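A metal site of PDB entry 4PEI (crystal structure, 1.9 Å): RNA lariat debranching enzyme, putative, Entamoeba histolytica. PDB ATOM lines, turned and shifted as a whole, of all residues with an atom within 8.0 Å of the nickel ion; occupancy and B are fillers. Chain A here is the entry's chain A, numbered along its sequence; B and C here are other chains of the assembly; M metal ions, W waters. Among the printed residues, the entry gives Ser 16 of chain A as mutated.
OE2 of Glu 94 lies within hydrogen-bond range of N of Asp 47, at 2.8 Å.
OD1 of Asp 47 sits at hydrogen-bond distance from N of His 93, at 3.0 Å.
O3P of G46 1 of chain B is bonded to C2' of A 3 of chain C (1.4 Å).
The side-chain amide nitrogen (ND2) of Asn 92 lies close to a ring nitrogen (NE2) of His 93, at 3.5 Å.
A ring nitrogen (NE2) of His 18 is in hydrogen-bond range of S2P of G46 1 of chain B (2.7 Å).
O3' of G46 1 of chain B is in hydrogen-bond range of ND1 of His 234.
A ring nitrogen (ND1) of His 182 is in hydrogen-bond range of the backbone carbonyl oxygen (O) of Thr 45.
S2P of G46 1 of chain B lies close to a ring nitrogen (NE2) of His 93, at 3.8 Å.
Within 4 Å of the nickel ion: Asp 47, Asn 92, His 182, His 232 and G46 1 of chain B.
The nickel ion is bound by NE2 of His 182, at 2.1 Å.
OD1 of Asn 92 is bound to the nickel ion, at 2.2 Å.
The nickel ion is bound by O1P of G46 1 of chain B (2.3 Å).
The nickel ion is bound by OD2 of Asp 47 (2.3 Å).
ND1 of His 232 is bound to the nickel ion (2.4 Å).
Water W1 binds the nickel ion (2.4 Å).
The nickel ion has six donor atoms within binding distance.
Water W1 lies within hydrogen-bond range of OG of Ser 16 (2.7 Å), O of His 232 (2.9 Å), S2P of G46 1 of chain B (3.3 Å) and NE2 of His 234 (3.4 Å).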
ATOM      1  N   SER A  16     -24.216  -2.031  -9.854  1.00  0.00           N
ATOM      2  CA  SER A  16     -24.361  -1.070  -8.746  1.00  0.00           C
ATOM      3  C   SER A  16     -25.804  -0.891  -8.246  1.00  0.00           C
ATOM      4  O   SER A  16     -26.699  -0.485  -9.019  1.00  0.00           O
ATOM      5  CB  SER A  16     -23.787   0.292  -9.125  1.00  0.00           C
ATOM      6  OG  SER A  16     -22.442   0.201  -9.566  1.00  0.00           O
ATOM      7  N   HIS A  18     -26.943   1.211  -5.571  1.00  0.00           N
ATOM      8  CA  HIS A  18     -27.178   2.618  -5.230  1.00  0.00           C
ATOM      9  C   HIS A  18     -28.455   2.848  -4.418  1.00  0.00           C
ATOM     10  O   HIS A  18     -29.184   3.844  -4.625  1.00  0.00           O
ATOM     11  CB  HIS A  18     -27.199   3.476  -6.505  1.00  0.00           C
ATOM     12  CG  HIS A  18     -25.858   3.653  -7.129  1.00  0.00           C
ATOM     13  ND1 HIS A  18     -24.809   4.280  -6.487  1.00  0.00           N
ATOM     14  CD2 HIS A  18     -25.367   3.263  -8.336  1.00  0.00           C
ATOM     15  CE1 HIS A  18     -23.743   4.268  -7.260  1.00  0.00           C
ATOM     16  NE2 HIS A  18     -24.050   3.666  -8.402  1.00  0.00           N
ATOM     17  N   THR A  45     -22.289  -6.446  -6.874  1.00  0.00           N
ATOM     18  CA  THR A  45     -20.883  -6.082  -6.965  1.00  0.00           C
ATOM     19  C   THR A  45     -20.607  -4.681  -6.434  1.00  0.00           C
ATOM     20  O   THR A  45     -19.571  -4.094  -6.751  1.00  0.00           O
ATOM     21  CB  THR A  45     -20.442  -6.064  -8.442  1.00  0.00           C
ATOM     22  OG1 THR A  45     -21.389  -5.299  -9.194  1.00  0.00           O
ATOM     23  CG2 THR A  45     -20.341  -7.442  -9.030  1.00  0.00           C
ATOM     24  N   GLY A  46     -21.528  -4.118  -5.651  1.00  0.00           N
ATOM     25  CA  GLY A  46     -21.156  -2.903  -4.930  1.00  0.00           C
ATOM     26  C   GLY A  46     -22.018  -1.653  -5.058  1.00  0.00           C
ATOM     27  O   GLY A  46     -23.097  -1.705  -5.674  1.00  0.00           O
ATOM     28  N   ASP A  47     -21.530  -0.566  -4.437  1.00  0.00           N
ATOM     29  CA  ASP A  47     -22.274   0.660  -4.170  1.00  0.00           C
ATOM     30  C   ASP A  47     -23.608   0.320  -3.552  1.00  0.00           C
ATOM     31  O   ASP A  47     -24.666   0.727  -4.077  1.00  0.00           O
ATOM     32  CB  ASP A  47     -22.418   1.505  -5.451  1.00  0.00           C
ATOM     33  CG  ASP A  47     -21.080   1.969  -6.002  1.00  0.00           C
ATOM     34  OD1 ASP A  47     -20.090   1.903  -5.255  1.00  0.00           O
ATOM     35  OD2 ASP A  47     -21.022   2.407  -7.186  1.00  0.00           O
ATOM     36  N   MET A  48     -23.555  -0.456  -2.457  1.00  0.00           N
ATOM     37  CA  MET A  48     -24.753  -0.917  -1.755  1.00  0.00           C
ATOM     38  C   MET A  48     -25.453   0.194  -0.953  1.00  0.00           C
ATOM     39  O   MET A  48     -26.651   0.146  -0.772  1.00  0.00           O
ATOM     40  CB  MET A  48     -24.445  -2.155  -0.891  1.00  0.00           C
ATOM     41  CG  MET A  48     -23.647  -3.228  -1.661  1.00  0.00           C
ATOM     42  SD  MET A  48     -24.550  -3.790  -3.143  1.00  0.00           S
ATOM     43  CE  MET A  48     -25.953  -4.525  -2.331  1.00  0.00           C
ATOM     44  N   GLN A  49     -24.721   1.183  -0.473  1.00  0.00           N
ATOM     45  CA  GLN A  49     -25.339   2.309   0.259  1.00  0.00           C
ATOM     46  C   GLN A  49     -26.284   1.851   1.371  1.00  0.00           C
ATOM     47  O   GLN A  49     -27.472   2.244   1.443  1.00  0.00           O
ATOM     48  CB  GLN A  49     -26.050   3.268  -0.737  1.00  0.00           C
ATOM     49  CG  GLN A  49     -25.088   3.663  -1.853  1.00  0.00           C
ATOM     50  CD  GLN A  49     -25.612   4.749  -2.800  1.00  0.00           C
ATOM     51  OE1 GLN A  49     -25.001   4.996  -3.860  1.00  0.00           O
ATOM     52  NE2 GLN A  49     -26.716   5.380  -2.425  1.00  0.00           N
ATOM     53  N   GLY A  90     -18.304  -4.289  -1.057  1.00  0.00           N
ATOM     54  CA  GLY A  90     -18.463  -2.836  -1.062  1.00  0.00           C
ATOM     55  C   GLY A  90     -17.865  -2.256  -2.338  1.00  0.00           C
ATOM     56  O   GLY A  90     -16.913  -2.829  -2.932  1.00  0.00           O
ATOM     57  N   GLY A  91     -18.413  -1.124  -2.766  1.00  0.00           N
ATOM     58  CA  GLY A  91     -17.840  -0.359  -3.865  1.00  0.00           C
ATOM     59  C   GLY A  91     -17.334   0.973  -3.317  1.00  0.00           C
ATOM     60  O   GLY A  91     -16.613   1.032  -2.300  1.00  0.00           O
ATOM     61  N   ASN A  92     -17.683   2.068  -3.972  1.00  0.00           N
ATOM     62  CA  ASN A  92     -17.100   3.364  -3.571  1.00  0.00           C
ATOM     63  C   ASN A  92     -18.164   4.322  -3.062  1.00  0.00           C
ATOM     64  O   ASN A  92     -17.828   5.436  -2.616  1.00  0.00           O
ATOM     65  CB  ASN A  92     -16.303   4.008  -4.732  1.00  0.00           C
ATOM     66  CG  ASN A  92     -17.162   4.263  -5.942  1.00  0.00           C
ATOM     67  OD1 ASN A  92     -17.606   3.302  -6.578  1.00  0.00           O
ATOM     68  ND2 ASN A  92     -17.390   5.535  -6.304  1.00  0.00           N
ATOM     69  N   HIS A  93     -19.419   3.867  -3.124  1.00  0.00           N
ATOM     70  CA  HIS A  93     -20.539   4.627  -2.615  1.00  0.00           C
ATOM     71  C   HIS A  93     -21.202   3.781  -1.522  1.00  0.00           C
ATOM     72  O   HIS A  93     -22.013   2.921  -1.803  1.00  0.00           O
ATOM     73  CB  HIS A  93     -21.554   4.871  -3.746  1.00  0.00           C
ATOM     74  CG  HIS A  93     -21.067   5.800  -4.817  1.00  0.00           C
ATOM     75  ND1 HIS A  93     -20.344   6.944  -4.558  1.00  0.00           N
ATOM     76  CD2 HIS A  93     -21.211   5.750  -6.173  1.00  0.00           C
ATOM     77  CE1 HIS A  93     -20.053   7.556  -5.691  1.00  0.00           C
ATOM     78  NE2 HIS A  93     -20.587   6.858  -6.691  1.00  0.00           N
ATOM     79  N   GLU A  94     -20.790   3.987  -0.271  1.00  0.00           N
ATOM     80  CA  GLU A  94     -21.178   3.029   0.767  1.00  0.00           C
ATOM     81  C   GLU A  94     -21.343   3.799   2.032  1.00  0.00           C
ATOM     82  O   GLU A  94     -20.782   4.896   2.165  1.00  0.00           O
ATOM     83  CB  GLU A  94     -20.074   1.961   0.966  1.00  0.00           C
ATOM     84  CG  GLU A  94     -19.781   1.076  -0.255  1.00  0.00           C
ATOM     85  CD  GLU A  94     -20.977   0.176  -0.647  1.00  0.00           C
ATOM     86  OE1 GLU A  94     -21.986   0.115   0.124  1.00  0.00           O
ATOM     87  OE2 GLU A  94     -20.870  -0.504  -1.690  1.00  0.00           O
ATOM     88  N   GLY A 133     -14.184  -2.372  -2.476  1.00  0.00           N
ATOM     89  CA  GLY A 133     -13.541  -1.087  -2.736  1.00  0.00           C
ATOM     90  C   GLY A 133     -13.148  -0.798  -4.186  1.00  0.00           C
ATOM     91  O   GLY A 133     -13.333  -1.619  -5.111  1.00  0.00           O
ATOM     92  N   ILE A 134     -12.602   0.393  -4.380  1.00  0.00           N
ATOM     93  CA  ILE A 134     -11.931   0.732  -5.606  1.00  0.00           C
ATOM     94  C   ILE A 134     -10.510   1.189  -5.274  1.00  0.00           C
ATOM     95  O   ILE A 134     -10.185   1.595  -4.132  1.00  0.00           O
ATOM     96  CB  ILE A 134     -12.672   1.839  -6.387  1.00  0.00           C
ATOM     97  CG1 ILE A 134     -12.661   3.137  -5.586  1.00  0.00           C
ATOM     98  CG2 ILE A 134     -14.126   1.447  -6.672  1.00  0.00           C
ATOM     99  CD1 ILE A 134     -13.113   4.361  -6.447  1.00  0.00           C
ATOM    100  N   HIS A 182     -15.467  -4.501  -7.325  1.00  0.00           N
ATOM    101  CA  HIS A 182     -16.178  -3.322  -7.764  1.00  0.00           C
ATOM    102  C   HIS A 182     -15.531  -2.754  -9.028  1.00  0.00           C
ATOM    103  O   HIS A 182     -16.081  -2.920 -10.095  1.00  0.00           O
ATOM    104  CB  HIS A 182     -16.391  -2.300  -6.645  1.00  0.00           C
ATOM    105  CG  HIS A 182     -17.386  -1.241  -7.028  1.00  0.00           C
ATOM    106  ND1 HIS A 182     -18.678  -1.559  -7.334  1.00  0.00           N
ATOM    107  CD2 HIS A 182     -17.224   0.077  -7.275  1.00  0.00           C
ATOM    108  CE1 HIS A 182     -19.322  -0.438  -7.679  1.00  0.00           C
ATOM    109  NE2 HIS A 182     -18.458   0.541  -7.676  1.00  0.00           N
ATOM    110  N   ASP A 183     -14.346  -2.161  -8.927  1.00  0.00           N
ATOM    111  CA  ASP A 183     -13.724  -1.700 -10.162  1.00  0.00           C
ATOM    112  C   ASP A 183     -13.178  -2.920 -10.906  1.00  0.00           C
ATOM    113  O   ASP A 183     -13.006  -4.020 -10.304  1.00  0.00           O
ATOM    114  CB  ASP A 183     -12.678  -0.587  -9.982  1.00  0.00           C
ATOM    115  CG  ASP A 183     -11.665  -0.870  -8.883  1.00  0.00           C
ATOM    116  OD1 ASP A 183     -11.723  -1.945  -8.236  1.00  0.00           O
ATOM    117  OD2 ASP A 183     -10.764  -0.027  -8.683  1.00  0.00           O
ATOM    118  N   GLY A 231     -18.806  -4.250 -11.098  1.00  0.00           N
ATOM    119  CA  GLY A 231     -19.924  -3.311 -11.234  1.00  0.00           C
ATOM    120  C   GLY A 231     -19.777  -1.768 -11.263  1.00  0.00           C
ATOM    121  O   GLY A 231     -20.741  -1.077 -11.517  1.00  0.00           O
ATOM    122  N   HIS A 232     -18.599  -1.253 -10.956  1.00  0.00           N
ATOM    123  CA  HIS A 232     -18.237   0.191 -11.064  1.00  0.00           C
ATOM    124  C   HIS A 232     -18.606   1.037 -12.316  1.00  0.00           C
ATOM    125  O   HIS A 232     -18.935   2.219 -12.175  1.00  0.00           O
ATOM    126  CB  HIS A 232     -16.760   0.341 -10.722  1.00  0.00           C
ATOM    127  CG  HIS A 232     -16.331   1.739 -10.420  1.00  0.00           C
ATOM    128  ND1 HIS A 232     -17.076   2.602  -9.635  1.00  0.00           N
ATOM    129  CD2 HIS A 232     -15.214   2.420 -10.760  1.00  0.00           C
ATOM    130  CE1 HIS A 232     -16.450   3.747  -9.526  1.00  0.00           C
ATOM    131  NE2 HIS A 232     -15.313   3.669 -10.198  1.00  0.00           N
ATOM    132  N   MET A 233     -18.574   0.441 -13.502  1.00  0.00           N
ATOM    133  CA  MET A 233     -18.505   1.228 -14.760  1.00  0.00           C
ATOM    134  C   MET A 233     -19.810   1.716 -15.445  1.00  0.00           C
ATOM    135  O   MET A 233     -19.758   2.566 -16.350  1.00  0.00           O
ATOM    136  CB  MET A 233     -17.620   0.521 -15.802  1.00  0.00           C
ATOM    137  CG  MET A 233     -16.155   0.332 -15.375  1.00  0.00           C
ATOM    138  SD  MET A 233     -15.312   1.820 -14.766  1.00  0.00           S
ATOM    139  CE  MET A 233     -14.949   2.632 -16.338  1.00  0.00           C
ATOM    140  N   HIS A 234     -20.962   1.189 -15.048  1.00  0.00           N
ATOM    141  CA  HIS A 234     -22.238   1.590 -15.655  1.00  0.00           C
ATOM    142  C   HIS A 234     -22.346   1.170 -17.104  1.00  0.00           C
ATOM    143  O   HIS A 234     -22.731   1.967 -17.960  1.00  0.00           O
ATOM    144  CB  HIS A 234     -22.443   3.094 -15.576  1.00  0.00           C
ATOM    145  CG  HIS A 234     -22.506   3.617 -14.183  1.00  0.00           C
ATOM    146  ND1 HIS A 234     -22.614   4.964 -13.895  1.00  0.00           N
ATOM    147  CD2 HIS A 234     -22.477   2.982 -12.984  1.00  0.00           C
ATOM    148  CE1 HIS A 234     -22.643   5.132 -12.591  1.00  0.00           C
ATOM    149  NE2 HIS A 234     -22.560   3.943 -12.005  1.00  0.00           N
ATOM    150  P   G46 B   1     -20.213   5.675  -9.553  1.00  0.00           P
ATOM    151  O1P G46 B   1     -19.412   4.709  -8.761  1.00  0.00           O
ATOM    152  S2P G46 B   1     -22.208   5.164  -9.620  1.00  0.00           S
ATOM    153  O3P G46 B   1     -20.036   7.142  -8.926  1.00  0.00           O
ATOM    154  O5' G46 B   1     -19.688   5.720 -11.071  1.00  0.00           O
ATOM    155  C5' G46 B   1     -18.505   6.436 -11.399  1.00  0.00           C
ATOM    156  C4' G46 B   1     -18.590   6.717 -12.892  1.00  0.00           C
ATOM    157  O4' G46 B   1     -17.292   7.065 -13.382  1.00  0.00           O
ATOM    158  C3' G46 B   1     -19.062   5.493 -13.656  1.00  0.00           C
ATOM    159  O3' G46 B   1     -20.313   5.803 -14.306  1.00  0.00           O
ATOM    160  C2' G46 B   1     -17.944   5.152 -14.645  1.00  0.00           C
ATOM    161  C1' G46 B   1     -16.918   6.278 -14.522  1.00  0.00           C
ATOM    162  O2' G46 B   1     -18.436   5.051 -15.992  1.00  0.00           O
ATOM    163  N9  G46 B   1     -15.559   5.775 -14.198  1.00  0.00           N
ATOM    164  C8  G46 B   1     -15.240   5.127 -13.059  1.00  0.00           C
ATOM    165  N7  G46 B   1     -13.921   4.792 -13.041  1.00  0.00           N
ATOM    166  C5  G46 B   1     -13.368   5.236 -14.178  1.00  0.00           C
ATOM    167  C6  G46 B   1     -11.999   5.210 -14.784  1.00  0.00           C
ATOM    168  O6  G46 B   1     -11.021   4.667 -14.205  1.00  0.00           O
ATOM    169  N1  G46 B   1     -11.857   5.786 -15.989  1.00  0.00           N
ATOM    170  C2  G46 B   1     -12.880   6.367 -16.648  1.00  0.00           C
ATOM    171  N2  G46 B   1     -12.607   6.925 -17.857  1.00  0.00           N
ATOM    172  N3  G46 B   1     -14.158   6.432 -16.155  1.00  0.00           N
ATOM    173  C4  G46 B   1     -14.455   5.881 -14.944  1.00  0.00           C
ATOM    174  C4'   A C   3     -20.668  10.610  -9.703  1.00  0.00           C
ATOM    175  O4'   A C   3     -21.664  10.268  -8.720  1.00  0.00           O
ATOM    176  C3'   A C   3     -19.666   9.474  -9.619  1.00  0.00           C
ATOM    177  O3'   A C   3     -18.931   9.668  -8.409  1.00  0.00           O
ATOM    178  C2'   A C   3     -20.618   8.297  -9.491  1.00  0.00           C
ATOM    179  C1'   A C   3     -21.669   8.869  -8.517  1.00  0.00           C
ATOM    180  N9    A C   3     -23.050   8.434  -8.692  1.00  0.00           N
ATOM    181  C8    A C   3     -23.764   8.400  -9.864  1.00  0.00           C
ATOM    182  N7    A C   3     -24.995   7.968  -9.726  1.00  0.00           N
ATOM    183  C5    A C   3     -25.110   7.693  -8.377  1.00  0.00           C
ATOM    184  C6    A C   3     -26.190   7.197  -7.594  1.00  0.00           C
ATOM    185  N6    A C   3     -27.389   6.886  -8.106  1.00  0.00           N
ATOM    186  N1    A C   3     -25.984   7.038  -6.261  1.00  0.00           N
ATOM    187  C2    A C   3     -24.770   7.357  -5.781  1.00  0.00           C
ATOM    188  N3    A C   3     -23.684   7.831  -6.412  1.00  0.00           N
ATOM    189  C4    A C   3     -23.922   7.986  -7.717  1.00  0.00           C
ATOM    190  P     C C   4     -17.389  10.149  -8.456  1.00  0.00           P
ATOM    191  OP1   C C   4     -16.948  10.335  -7.045  1.00  0.00           O
ATOM    192  OP2   C C   4     -17.235  11.259  -9.440  1.00  0.00           O
ATOM    193  O5'   C C   4     -16.627   8.878  -9.038  1.00  0.00           O
ATOM    194  C5'   C C   4     -16.397   7.725  -8.247  1.00  0.00           C
ATOM    195  C4'   C C   4     -14.929   7.423  -8.110  1.00  0.00           C
ATOM    196  O4'   C C   4     -14.397   7.120  -9.428  1.00  0.00           O
ATOM    197  C3'   C C   4     -14.086   8.561  -7.550  1.00  0.00           C
ATOM    198  O3'   C C   4     -13.051   8.032  -6.716  1.00  0.00           O
ATOM    199  C2'   C C   4     -13.457   9.180  -8.792  1.00  0.00           C
ATOM    200  O2'   C C   4     -12.224   9.835  -8.555  1.00  0.00           O
ATOM    201  C1'   C C   4     -13.285   7.963  -9.698  1.00  0.00           C
HETATM  202 NI    NI M   1     -18.944   2.549  -8.200  1.00  0.00          NI
HETATM  203  O   HOH W   1     -20.645   2.253  -9.809  1.00  0.00           O
